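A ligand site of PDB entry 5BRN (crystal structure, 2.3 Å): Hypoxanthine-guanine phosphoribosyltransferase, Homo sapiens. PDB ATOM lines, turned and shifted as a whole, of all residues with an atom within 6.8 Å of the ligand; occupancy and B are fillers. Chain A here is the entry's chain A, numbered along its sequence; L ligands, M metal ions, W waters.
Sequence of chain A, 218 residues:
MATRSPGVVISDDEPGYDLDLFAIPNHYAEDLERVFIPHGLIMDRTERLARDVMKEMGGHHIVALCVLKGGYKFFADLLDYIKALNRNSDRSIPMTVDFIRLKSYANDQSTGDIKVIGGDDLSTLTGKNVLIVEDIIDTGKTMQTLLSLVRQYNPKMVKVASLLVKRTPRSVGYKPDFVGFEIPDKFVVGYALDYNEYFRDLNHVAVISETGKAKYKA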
ATOM      1  N   GLY A  70      18.952 -22.801 -19.110  1.00  0.00           N
ATOM      2  CA  GLY A  70      18.707 -21.382 -18.956  1.00  0.00           C
ATOM      3  C   GLY A  70      17.249 -20.961 -19.030  1.00  0.00           C
ATOM      4  O   GLY A  70      16.849 -19.990 -18.380  1.00  0.00           O
ATOM      5  N   LEU A 102      20.890 -27.983 -25.963  1.00  0.00           N
ATOM      6  CA  LEU A 102      21.811 -27.871 -27.091  1.00  0.00           C
ATOM      7  C   LEU A 102      23.231 -27.580 -26.614  1.00  0.00           C
ATOM      8  O   LEU A 102      23.501 -26.496 -26.097  1.00  0.00           O
ATOM      9  CB  LEU A 102      21.356 -26.793 -28.071  1.00  0.00           C
ATOM     10  CG  LEU A 102      20.181 -27.133 -28.998  1.00  0.00           C
ATOM     11  CD1 LEU A 102      18.843 -26.867 -28.324  1.00  0.00           C
ATOM     12  CD2 LEU A 102      20.294 -26.372 -30.314  1.00  0.00           C
ATOM     13  N   GLU A 134      12.875 -20.043 -24.679  1.00  0.00           N
ATOM     14  CA  GLU A 134      14.307 -19.851 -24.565  1.00  0.00           C
ATOM     15  C   GLU A 134      14.668 -18.681 -23.648  1.00  0.00           C
ATOM     16  O   GLU A 134      13.888 -17.739 -23.504  1.00  0.00           O
ATOM     17  CB  GLU A 134      14.916 -19.650 -25.963  1.00  0.00           C
ATOM     18  CG  GLU A 134      16.410 -19.333 -26.008  1.00  0.00           C
ATOM     19  CD  GLU A 134      17.296 -20.524 -25.684  1.00  0.00           C
ATOM     20  OE1 GLU A 134      17.094 -21.165 -24.633  1.00  0.00           O
ATOM     21  OE2 GLU A 134      18.212 -20.805 -26.480  1.00  0.00           O
ATOM     22  N   ASP A 135      15.829 -18.760 -23.009  1.00  0.00           N
ATOM     23  CA  ASP A 135      16.286 -17.704 -22.120  1.00  0.00           C
ATOM     24  C   ASP A 135      16.868 -16.499 -22.862  1.00  0.00           C
ATOM     25  O   ASP A 135      16.543 -15.354 -22.539  1.00  0.00           O
ATOM     26  CB  ASP A 135      17.327 -18.256 -21.136  1.00  0.00           C
ATOM     27  CG  ASP A 135      18.517 -18.881 -21.826  1.00  0.00           C
ATOM     28  OD1 ASP A 135      18.424 -19.177 -23.039  1.00  0.00           O
ATOM     29  OD2 ASP A 135      19.561 -19.070 -21.167  1.00  0.00           O
ATOM     30  N   ILE A 136      17.719 -16.743 -23.843  1.00  0.00           N
ATOM     31  CA  ILE A 136      18.407 -15.641 -24.516  1.00  0.00           C
ATOM     32  C   ILE A 136      18.830 -15.957 -25.959  1.00  0.00           C
ATOM     33  O   ILE A 136      19.315 -17.046 -26.262  1.00  0.00           O
ATOM     34  CB  ILE A 136      19.660 -15.212 -23.712  1.00  0.00           C
ATOM     35  CG1 ILE A 136      20.361 -14.026 -24.373  1.00  0.00           C
ATOM     36  CG2 ILE A 136      20.614 -16.379 -23.512  1.00  0.00           C
ATOM     37  CD1 ILE A 136      21.424 -13.401 -23.518  1.00  0.00           C
ATOM     38  N   ILE A 137      18.618 -14.984 -26.849  1.00  0.00           N
ATOM     39  CA  ILE A 137      19.061 -15.073 -28.223  1.00  0.00           C
ATOM     40  C   ILE A 137      20.151 -14.042 -28.503  1.00  0.00           C
ATOM     41  O   ILE A 137      19.959 -12.846 -28.301  1.00  0.00           O
ATOM     42  CB  ILE A 137      17.899 -14.863 -29.212  1.00  0.00           C
ATOM     43  CG1 ILE A 137      16.862 -15.978 -29.071  1.00  0.00           C
ATOM     44  CG2 ILE A 137      18.408 -14.793 -30.648  1.00  0.00           C
ATOM     45  CD1 ILE A 137      15.701 -15.857 -30.029  1.00  0.00           C
ATOM     46  N   ASP A 138      21.305 -14.518 -28.961  1.00  0.00           N
ATOM     47  CA  ASP A 138      22.443 -13.651 -29.217  1.00  0.00           C
ATOM     48  C   ASP A 138      22.784 -13.622 -30.708  1.00  0.00           C
ATOM     49  O   ASP A 138      22.362 -12.719 -31.432  1.00  0.00           O
ATOM     50  CB  ASP A 138      23.663 -14.103 -28.407  1.00  0.00           C
ATOM     51  CG  ASP A 138      24.763 -13.060 -28.348  1.00  0.00           C
ATOM     52  OD1 ASP A 138      24.703 -12.071 -29.105  1.00  0.00           O
ATOM     53  OD2 ASP A 138      25.703 -13.242 -27.538  1.00  0.00           O
ATOM     54  N   THR A 139      23.558 -14.608 -31.151  1.00  0.00           N
ATOM     55  CA  THR A 139      23.921 -14.729 -32.553  1.00  0.00           C
ATOM     56  C   THR A 139      22.758 -15.303 -33.358  1.00  0.00           C
ATOM     57  O   THR A 139      22.678 -15.119 -34.569  1.00  0.00           O
ATOM     58  CB  THR A 139      25.150 -15.612 -32.745  1.00  0.00           C
ATOM     59  OG1 THR A 139      24.895 -16.918 -32.208  1.00  0.00           O
ATOM     60  CG2 THR A 139      26.352 -15.010 -32.028  1.00  0.00           C
ATOM     61  N   GLY A 140      21.858 -15.994 -32.663  1.00  0.00           N
ATOM     62  CA  GLY A 140      20.692 -16.590 -33.297  1.00  0.00           C
ATOM     63  C   GLY A 140      20.939 -18.004 -33.768  1.00  0.00           C
ATOM     64  O   GLY A 140      20.014 -18.693 -34.203  1.00  0.00           O
ATOM     65  N   LYS A 141      22.194 -18.445 -33.660  1.00  0.00           N
ATOM     66  CA  LYS A 141      22.597 -19.766 -34.159  1.00  0.00           C
ATOM     67  C   LYS A 141      21.881 -20.910 -33.429  1.00  0.00           C
ATOM     68  O   LYS A 141      21.503 -21.897 -34.052  1.00  0.00           O
ATOM     69  CB  LYS A 141      24.103 -19.940 -34.030  1.00  0.00           C
ATOM     70  CG  LYS A 141      24.930 -18.900 -34.772  1.00  0.00           C
ATOM     71  CD  LYS A 141      26.379 -19.345 -34.906  1.00  0.00           C
ATOM     72  CE  LYS A 141      27.346 -18.261 -34.471  1.00  0.00           C
ATOM     73  NZ  LYS A 141      27.356 -18.085 -32.993  1.00  0.00           N
ATOM     74  N   THR A 142      21.718 -20.766 -32.116  1.00  0.00           N
ATOM     75  CA  THR A 142      21.083 -21.805 -31.317  1.00  0.00           C
ATOM     76  C   THR A 142      19.652 -22.076 -31.772  1.00  0.00           C
ATOM     77  O   THR A 142      19.247 -23.228 -31.938  1.00  0.00           O
ATOM     78  CB  THR A 142      21.072 -21.443 -29.817  1.00  0.00           C
ATOM     79  OG1 THR A 142      22.420 -21.288 -29.346  1.00  0.00           O
ATOM     80  CG2 THR A 142      20.375 -22.526 -29.008  1.00  0.00           C
ATOM     81  N   MET A 143      18.891 -21.010 -31.971  1.00  0.00           N
ATOM     82  CA  MET A 143      17.476 -21.146 -32.283  1.00  0.00           C
ATOM     83  C   MET A 143      17.222 -21.653 -33.703  1.00  0.00           C
ATOM     84  O   MET A 143      16.361 -22.497 -33.915  1.00  0.00           O
ATOM     85  CB  MET A 143      16.758 -19.808 -32.081  1.00  0.00           C
ATOM     86  CG  MET A 143      15.240 -19.935 -32.068  1.00  0.00           C
ATOM     87  SD  MET A 143      14.691 -21.242 -30.960  1.00  0.00           S
ATOM     88  CE  MET A 143      15.310 -20.627 -29.390  1.00  0.00           C
ATOM     89  N   LEU A 164      15.207 -12.800 -23.493  1.00  0.00           N
ATOM     90  CA  LEU A 164      16.136 -11.750 -23.865  1.00  0.00           C
ATOM     91  C   LEU A 164      16.582 -11.866 -25.322  1.00  0.00           C
ATOM     92  O   LEU A 164      16.876 -12.963 -25.801  1.00  0.00           O
ATOM     93  CB  LEU A 164      17.370 -11.776 -22.957  1.00  0.00           C
ATOM     94  CG  LEU A 164      17.134 -11.610 -21.450  1.00  0.00           C
ATOM     95  CD1 LEU A 164      18.447 -11.665 -20.695  1.00  0.00           C
ATOM     96  CD2 LEU A 164      16.403 -10.315 -21.158  1.00  0.00           C
ATOM     97  N   LYS A 166      19.447  -9.821 -27.730  1.00  0.00           N
ATOM     98  CA  LYS A 166      20.495  -8.822 -27.719  1.00  0.00           C
ATOM     99  C   LYS A 166      20.576  -8.062 -29.035  1.00  0.00           C
ATOM    100  O   LYS A 166      20.327  -8.614 -30.104  1.00  0.00           O
ATOM    101  CB  LYS A 166      21.849  -9.469 -27.427  1.00  0.00           C
ATOM    102  CG  LYS A 166      22.007  -9.950 -25.991  1.00  0.00           C
ATOM    103  CD  LYS A 166      23.419 -10.435 -25.725  1.00  0.00           C
ATOM    104  CE  LYS A 166      23.638 -10.732 -24.245  1.00  0.00           C
ATOM    105  NZ  LYS A 166      24.989 -11.290 -23.984  1.00  0.00           N
ATOM    106  N   ARG A 170      26.796  -9.498 -34.325  1.00  0.00           N
ATOM    107  CA  ARG A 170      27.080 -10.918 -34.514  1.00  0.00           C
ATOM    108  C   ARG A 170      25.814 -11.687 -34.867  1.00  0.00           C
ATOM    109  O   ARG A 170      25.862 -12.892 -35.142  1.00  0.00           O
ATOM    110  CB  ARG A 170      27.721 -11.506 -33.264  1.00  0.00           C
ATOM    111  CG  ARG A 170      29.129 -11.005 -32.979  1.00  0.00           C
ATOM    112  CD  ARG A 170      29.720 -11.689 -31.748  1.00  0.00           C
ATOM    113  NE  ARG A 170      28.905 -11.469 -30.564  1.00  0.00           N
ATOM    114  CZ  ARG A 170      28.532 -12.423 -29.718  1.00  0.00           C
ATOM    115  NH1 ARG A 170      28.897 -13.679 -29.942  1.00  0.00           N
ATOM    116  NH2 ARG A 170      27.789 -12.126 -28.663  1.00  0.00           N
ATOM    117  N   ILE A 183      17.835  -6.134 -25.251  1.00  0.00           N
ATOM    118  CA  ILE A 183      18.922  -5.543 -24.471  1.00  0.00           C
ATOM    119  C   ILE A 183      20.159  -5.246 -25.315  1.00  0.00           C
ATOM    120  O   ILE A 183      20.335  -5.823 -26.387  1.00  0.00           O
ATOM    121  CB  ILE A 183      19.310  -6.481 -23.311  1.00  0.00           C
ATOM    122  CG1 ILE A 183      19.793  -7.826 -23.858  1.00  0.00           C
ATOM    123  CG2 ILE A 183      18.147  -6.674 -22.353  1.00  0.00           C
ATOM    124  CD1 ILE A 183      20.059  -8.864 -22.787  1.00  0.00           C
ATOM    125  N   ASP A 185      24.253  -5.418 -26.184  1.00  0.00           N
ATOM    126  CA  ASP A 185      25.185  -6.539 -26.129  1.00  0.00           C
ATOM    127  C   ASP A 185      26.034  -6.461 -24.866  1.00  0.00           C
ATOM    128  O   ASP A 185      27.148  -5.944 -24.881  1.00  0.00           O
ATOM    129  CB  ASP A 185      26.078  -6.572 -27.371  1.00  0.00           C
ATOM    130  CG  ASP A 185      26.952  -7.814 -27.428  1.00  0.00           C
ATOM    131  OD1 ASP A 185      26.637  -8.798 -26.725  1.00  0.00           O
ATOM    132  OD2 ASP A 185      27.962  -7.796 -28.163  1.00  0.00           O
ATOM    133  N   LYS A 186      25.499  -6.991 -23.764  1.00  0.00           N
ATOM    134  CA  LYS A 186      26.210  -7.048 -22.496  1.00  0.00           C
ATOM    135  C   LYS A 186      25.924  -8.375 -21.811  1.00  0.00           C
ATOM    136  O   LYS A 186      24.808  -8.878 -21.868  1.00  0.00           O
ATOM    137  CB  LYS A 186      25.800  -5.881 -21.613  1.00  0.00           C
ATOM    138  N   PHE A 187      26.935  -8.946 -21.168  1.00  0.00           N
ATOM    139  CA  PHE A 187      26.789 -10.246 -20.537  1.00  0.00           C
ATOM    140  C   PHE A 187      25.997 -10.134 -19.229  1.00  0.00           C
ATOM    141  O   PHE A 187      26.372  -9.387 -18.328  1.00  0.00           O
ATOM    142  CB  PHE A 187      28.152 -10.880 -20.260  1.00  0.00           C
ATOM    143  CG  PHE A 187      28.079 -12.322 -19.844  1.00  0.00           C
ATOM    144  CD1 PHE A 187      28.087 -13.338 -20.780  1.00  0.00           C
ATOM    145  CD2 PHE A 187      27.994 -12.660 -18.501  1.00  0.00           C
ATOM    146  CE1 PHE A 187      28.014 -14.662 -20.402  1.00  0.00           C
ATOM    147  CE2 PHE A 187      27.918 -13.981 -18.109  1.00  0.00           C
ATOM    148  CZ  PHE A 187      27.935 -14.984 -19.061  1.00  0.00           C
ATOM    149  N   VAL A 188      24.905 -10.890 -19.140  1.00  0.00           N
ATOM    150  CA  VAL A 188      24.029 -10.831 -17.976  1.00  0.00           C
ATOM    151  C   VAL A 188      23.828 -12.220 -17.359  1.00  0.00           C
ATOM    152  O   VAL A 188      23.971 -13.237 -18.033  1.00  0.00           O
ATOM    153  CB  VAL A 188      22.662 -10.240 -18.333  1.00  0.00           C
ATOM    154  CG1 VAL A 188      22.789  -8.767 -18.697  1.00  0.00           C
ATOM    155  CG2 VAL A 188      22.022 -11.033 -19.464  1.00  0.00           C
ATOM    156  N   VAL A 189      23.512 -12.247 -16.072  1.00  0.00           N
ATOM    157  CA  VAL A 189      23.262 -13.497 -15.367  1.00  0.00           C
ATOM    158  C   VAL A 189      21.978 -13.408 -14.550  1.00  0.00           C
ATOM    159  O   VAL A 189      21.384 -12.334 -14.437  1.00  0.00           O
ATOM    160  CB  VAL A 189      24.424 -13.872 -14.434  1.00  0.00           C
ATOM    161  CG1 VAL A 189      25.668 -14.205 -15.237  1.00  0.00           C
ATOM    162  CG2 VAL A 189      24.701 -12.745 -13.437  1.00  0.00           C
ATOM    163  N   LEU A 193      19.766 -17.910 -16.042  1.00  0.00           N
ATOM    164  CA  LEU A 193      20.910 -17.672 -16.918  1.00  0.00           C
ATOM    165  C   LEU A 193      22.200 -17.810 -16.118  1.00  0.00           C
ATOM    166  O   LEU A 193      22.292 -17.334 -14.989  1.00  0.00           O
ATOM    167  CB  LEU A 193      20.839 -16.283 -17.569  1.00  0.00           C
ATOM    168  CG  LEU A 193      19.958 -16.142 -18.814  1.00  0.00           C
ATOM    169  CD1 LEU A 193      18.487 -16.019 -18.446  1.00  0.00           C
ATOM    170  CD2 LEU A 193      20.415 -14.958 -19.658  1.00  0.00           C
ATOM    171  N   ASP A 194      23.200 -18.466 -16.699  1.00  0.00           N
ATOM    172  CA  ASP A 194      24.390 -18.829 -15.942  1.00  0.00           C
ATOM    173  C   ASP A 194      25.666 -18.126 -16.368  1.00  0.00           C
ATOM    174  O   ASP A 194      25.778 -17.631 -17.489  1.00  0.00           O
ATOM    175  CB  ASP A 194      24.621 -20.344 -16.023  1.00  0.00           C
ATOM    176  CG  ASP A 194      25.305 -20.755 -17.313  1.00  0.00           C
ATOM    177  OD1 ASP A 194      24.855 -20.323 -18.398  1.00  0.00           O
ATOM    178  OD2 ASP A 194      26.298 -21.512 -17.252  1.00  0.00           O
ATOM    179  N   TYR A 195      26.616 -18.109 -15.447  1.00  0.00           N
ATOM    180  CA  TYR A 195      28.014 -17.815 -15.745  1.00  0.00           C
ATOM    181  C   TYR A 195      28.837 -19.001 -15.258  1.00  0.00           C
ATOM    182  O   TYR A 195      29.167 -19.087 -14.074  1.00  0.00           O
ATOM    183  CB  TYR A 195      28.477 -16.518 -15.089  1.00  0.00           C
ATOM    184  CG  TYR A 195      29.955 -16.241 -15.271  1.00  0.00           C
ATOM    185  CD1 TYR A 195      30.438 -15.727 -16.473  1.00  0.00           C
ATOM    186  CD2 TYR A 195      30.865 -16.479 -14.251  1.00  0.00           C
ATOM    187  CE1 TYR A 195      31.780 -15.467 -16.640  1.00  0.00           C
ATOM    188  CE2 TYR A 195      32.207 -16.223 -14.410  1.00  0.00           C
ATOM    189  CZ  TYR A 195      32.662 -15.718 -15.616  1.00  0.00           C
ATOM    190  OH  TYR A 195      34.004 -15.458 -15.784  1.00  0.00           O
HETATM  191  N1  LIG L   1      25.198 -16.585 -23.897  1.00  0.00           N
HETATM  192  C1  LIG L   1      24.965 -16.109 -22.619  1.00  0.00           C
HETATM  193  C2  LIG L   1      24.682 -15.933 -20.329  1.00  0.00           C
HETATM  194  C3  LIG L   1      24.448 -13.992 -21.555  1.00  0.00           C
HETATM  195  C4  LIG L   1      25.104 -15.573 -24.744  1.00  0.00           C
HETATM  196  O1  LIG L   1      22.007 -16.919 -30.364  1.00  0.00           O
HETATM  197  P1  LIG L   1      23.097 -17.635 -29.597  1.00  0.00           P
HETATM  198  O2  LIG L   1      24.395 -16.881 -29.766  1.00  0.00           O
HETATM  199  O3  LIG L   1      23.249 -19.041 -30.154  1.00  0.00           O
HETATM  200  C5  LIG L   1      22.645 -17.714 -27.813  1.00  0.00           C
HETATM  201  C6  LIG L   1      23.669 -18.472 -26.954  1.00  0.00           C
HETATM  202  O4  LIG L   1      23.544 -18.033 -25.616  1.00  0.00           O
HETATM  203  C7  LIG L   1      24.280 -18.768 -24.687  1.00  0.00           C
HETATM  204  C8  LIG L   1      23.431 -19.116 -23.472  1.00  0.00           C
HETATM  205  O5  LIG L   1      23.013 -20.481 -23.595  1.00  0.00           O
HETATM  206  C9  LIG L   1      25.512 -17.979 -24.243  1.00  0.00           C
HETATM  207  N2  LIG L   1      24.939 -16.667 -21.385  1.00  0.00           N
HETATM  208  N3  LIG L   1      24.443 -14.617 -20.381  1.00  0.00           N
HETATM  209  O6  LIG L   1      24.194 -12.591 -21.617  1.00  0.00           O
HETATM  210  C10 LIG L   1      24.723 -14.737 -22.754  1.00  0.00           C
HETATM  211  N4  LIG L   1      24.818 -14.442 -24.076  1.00  0.00           N
HETATM  212 MG    MG M   1      19.424 -21.153 -24.254  1.00  0.00          MG
HETATM  213  O   HOH W   1      20.573 -19.344 -25.281  1.00  0.00           O
HETATM  214  O   HOH W   2      26.427 -18.846 -20.111  1.00  0.00           O
HETATM  215  O   HOH W   3      19.619 -18.285 -30.564  1.00  0.00           O
HETATM  216  O   HOH W   4      20.679 -20.950 -22.684  1.00  0.00           O
HETATM  217  O   HOH W   5      22.436 -22.007 -26.374  1.00  0.00           O
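N of Thr 139 lies within hydrogen-bond range of O2 of the ligand, at 2.8 Å. The backbone NH of Thr 142 sits at hydrogen-bond distance from an oxygen (O3) of the ligand (3.0 Å). The backbone NH (N) of Asp 138 is in hydrogen-bond range of an oxygen (O1) of the ligand, at 2.9 Å. The side-chain amino group (NZ) of Lys 166 is in hydrogen-bond range of an oxygen (O6) of the ligand, at 2.8 Å. An oxygen (O1) of the ligand sits at hydrogen-bond distance from the backbone NH of Gly 140. OG1 of Thr 139 sits at hydrogen-bond distance from O2 of the ligand (2.5 Å). The side-chain hydroxyl of Thr 142 lies within hydrogen-bond range of an oxygen (O3) of the ligand, at 2.5 Å. O of Val 188 is in hydrogen-bond range of N3 of the ligand, 2.8 Å away. An oxygen (O6) of the ligand lies within hydrogen-bond range of the backbone NH (N) of Val 188, 3.1 Å away.
The guanidinium group of Arg 170 is in salt-bridge range of the side-chain carboxylate of Asp 138, 2.6 Å away. The side-chain amino group of Lys 141 sits at hydrogen-bond distance from the side-chain hydroxyl of Thr 139 (2.8 Å). The backbone carbonyl oxygen (O) of Ile 137 is in hydrogen-bond range of the backbone NH (N) of Lys 166, 3.1 Å away. The backbone NH (N) of Ile 137 is in hydrogen-bond range of the backbone carbonyl oxygen (O) of Leu 164. The side-chain amino group of Lys 166 sits at hydrogen-bond distance from the backbone carbonyl oxygen of Lys 186 (3.2 Å).
Merely in contact with the ligand: Ile 136 (3.5 Å), Ile 137 (3.9 Å), Lys 141 (3.6 Å), Lys 186 (3.8 Å), Phe 187 (3.6 Å) and Asp 194 (3.5 Å). Hydrophobic or aromatic side chains that line the ligand: Ile 136, Phe 187 and Val 188. 12 residues have an atom within 4 Å of the ligand: Ile 136, Ile 137, Asp 138, Thr 139, Gly 140, Lys 141, Thr 142, Lys 166, Lys 186, Phe 187, Val 188 and Asp 194.
Water W4 bridges O5 of the ligand (2.5 Å) and OD2 of Asp 135 (2.7 Å). Water W3 bridges an oxygen (O1) of the ligand and the backbone NH (N) of Met 143. Water W2 bridges the side-chain carboxylate of Asp 194 (2.8 Å) and a nitrogen (N2) of the ligand (2.9 Å). Water W1 lies within hydrogen-bond range of O of Ile 136 and O5 of the ligand. Water W5 bridges the side-chain hydroxyl of Thr 142 and an oxygen (O5) of the ligand.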
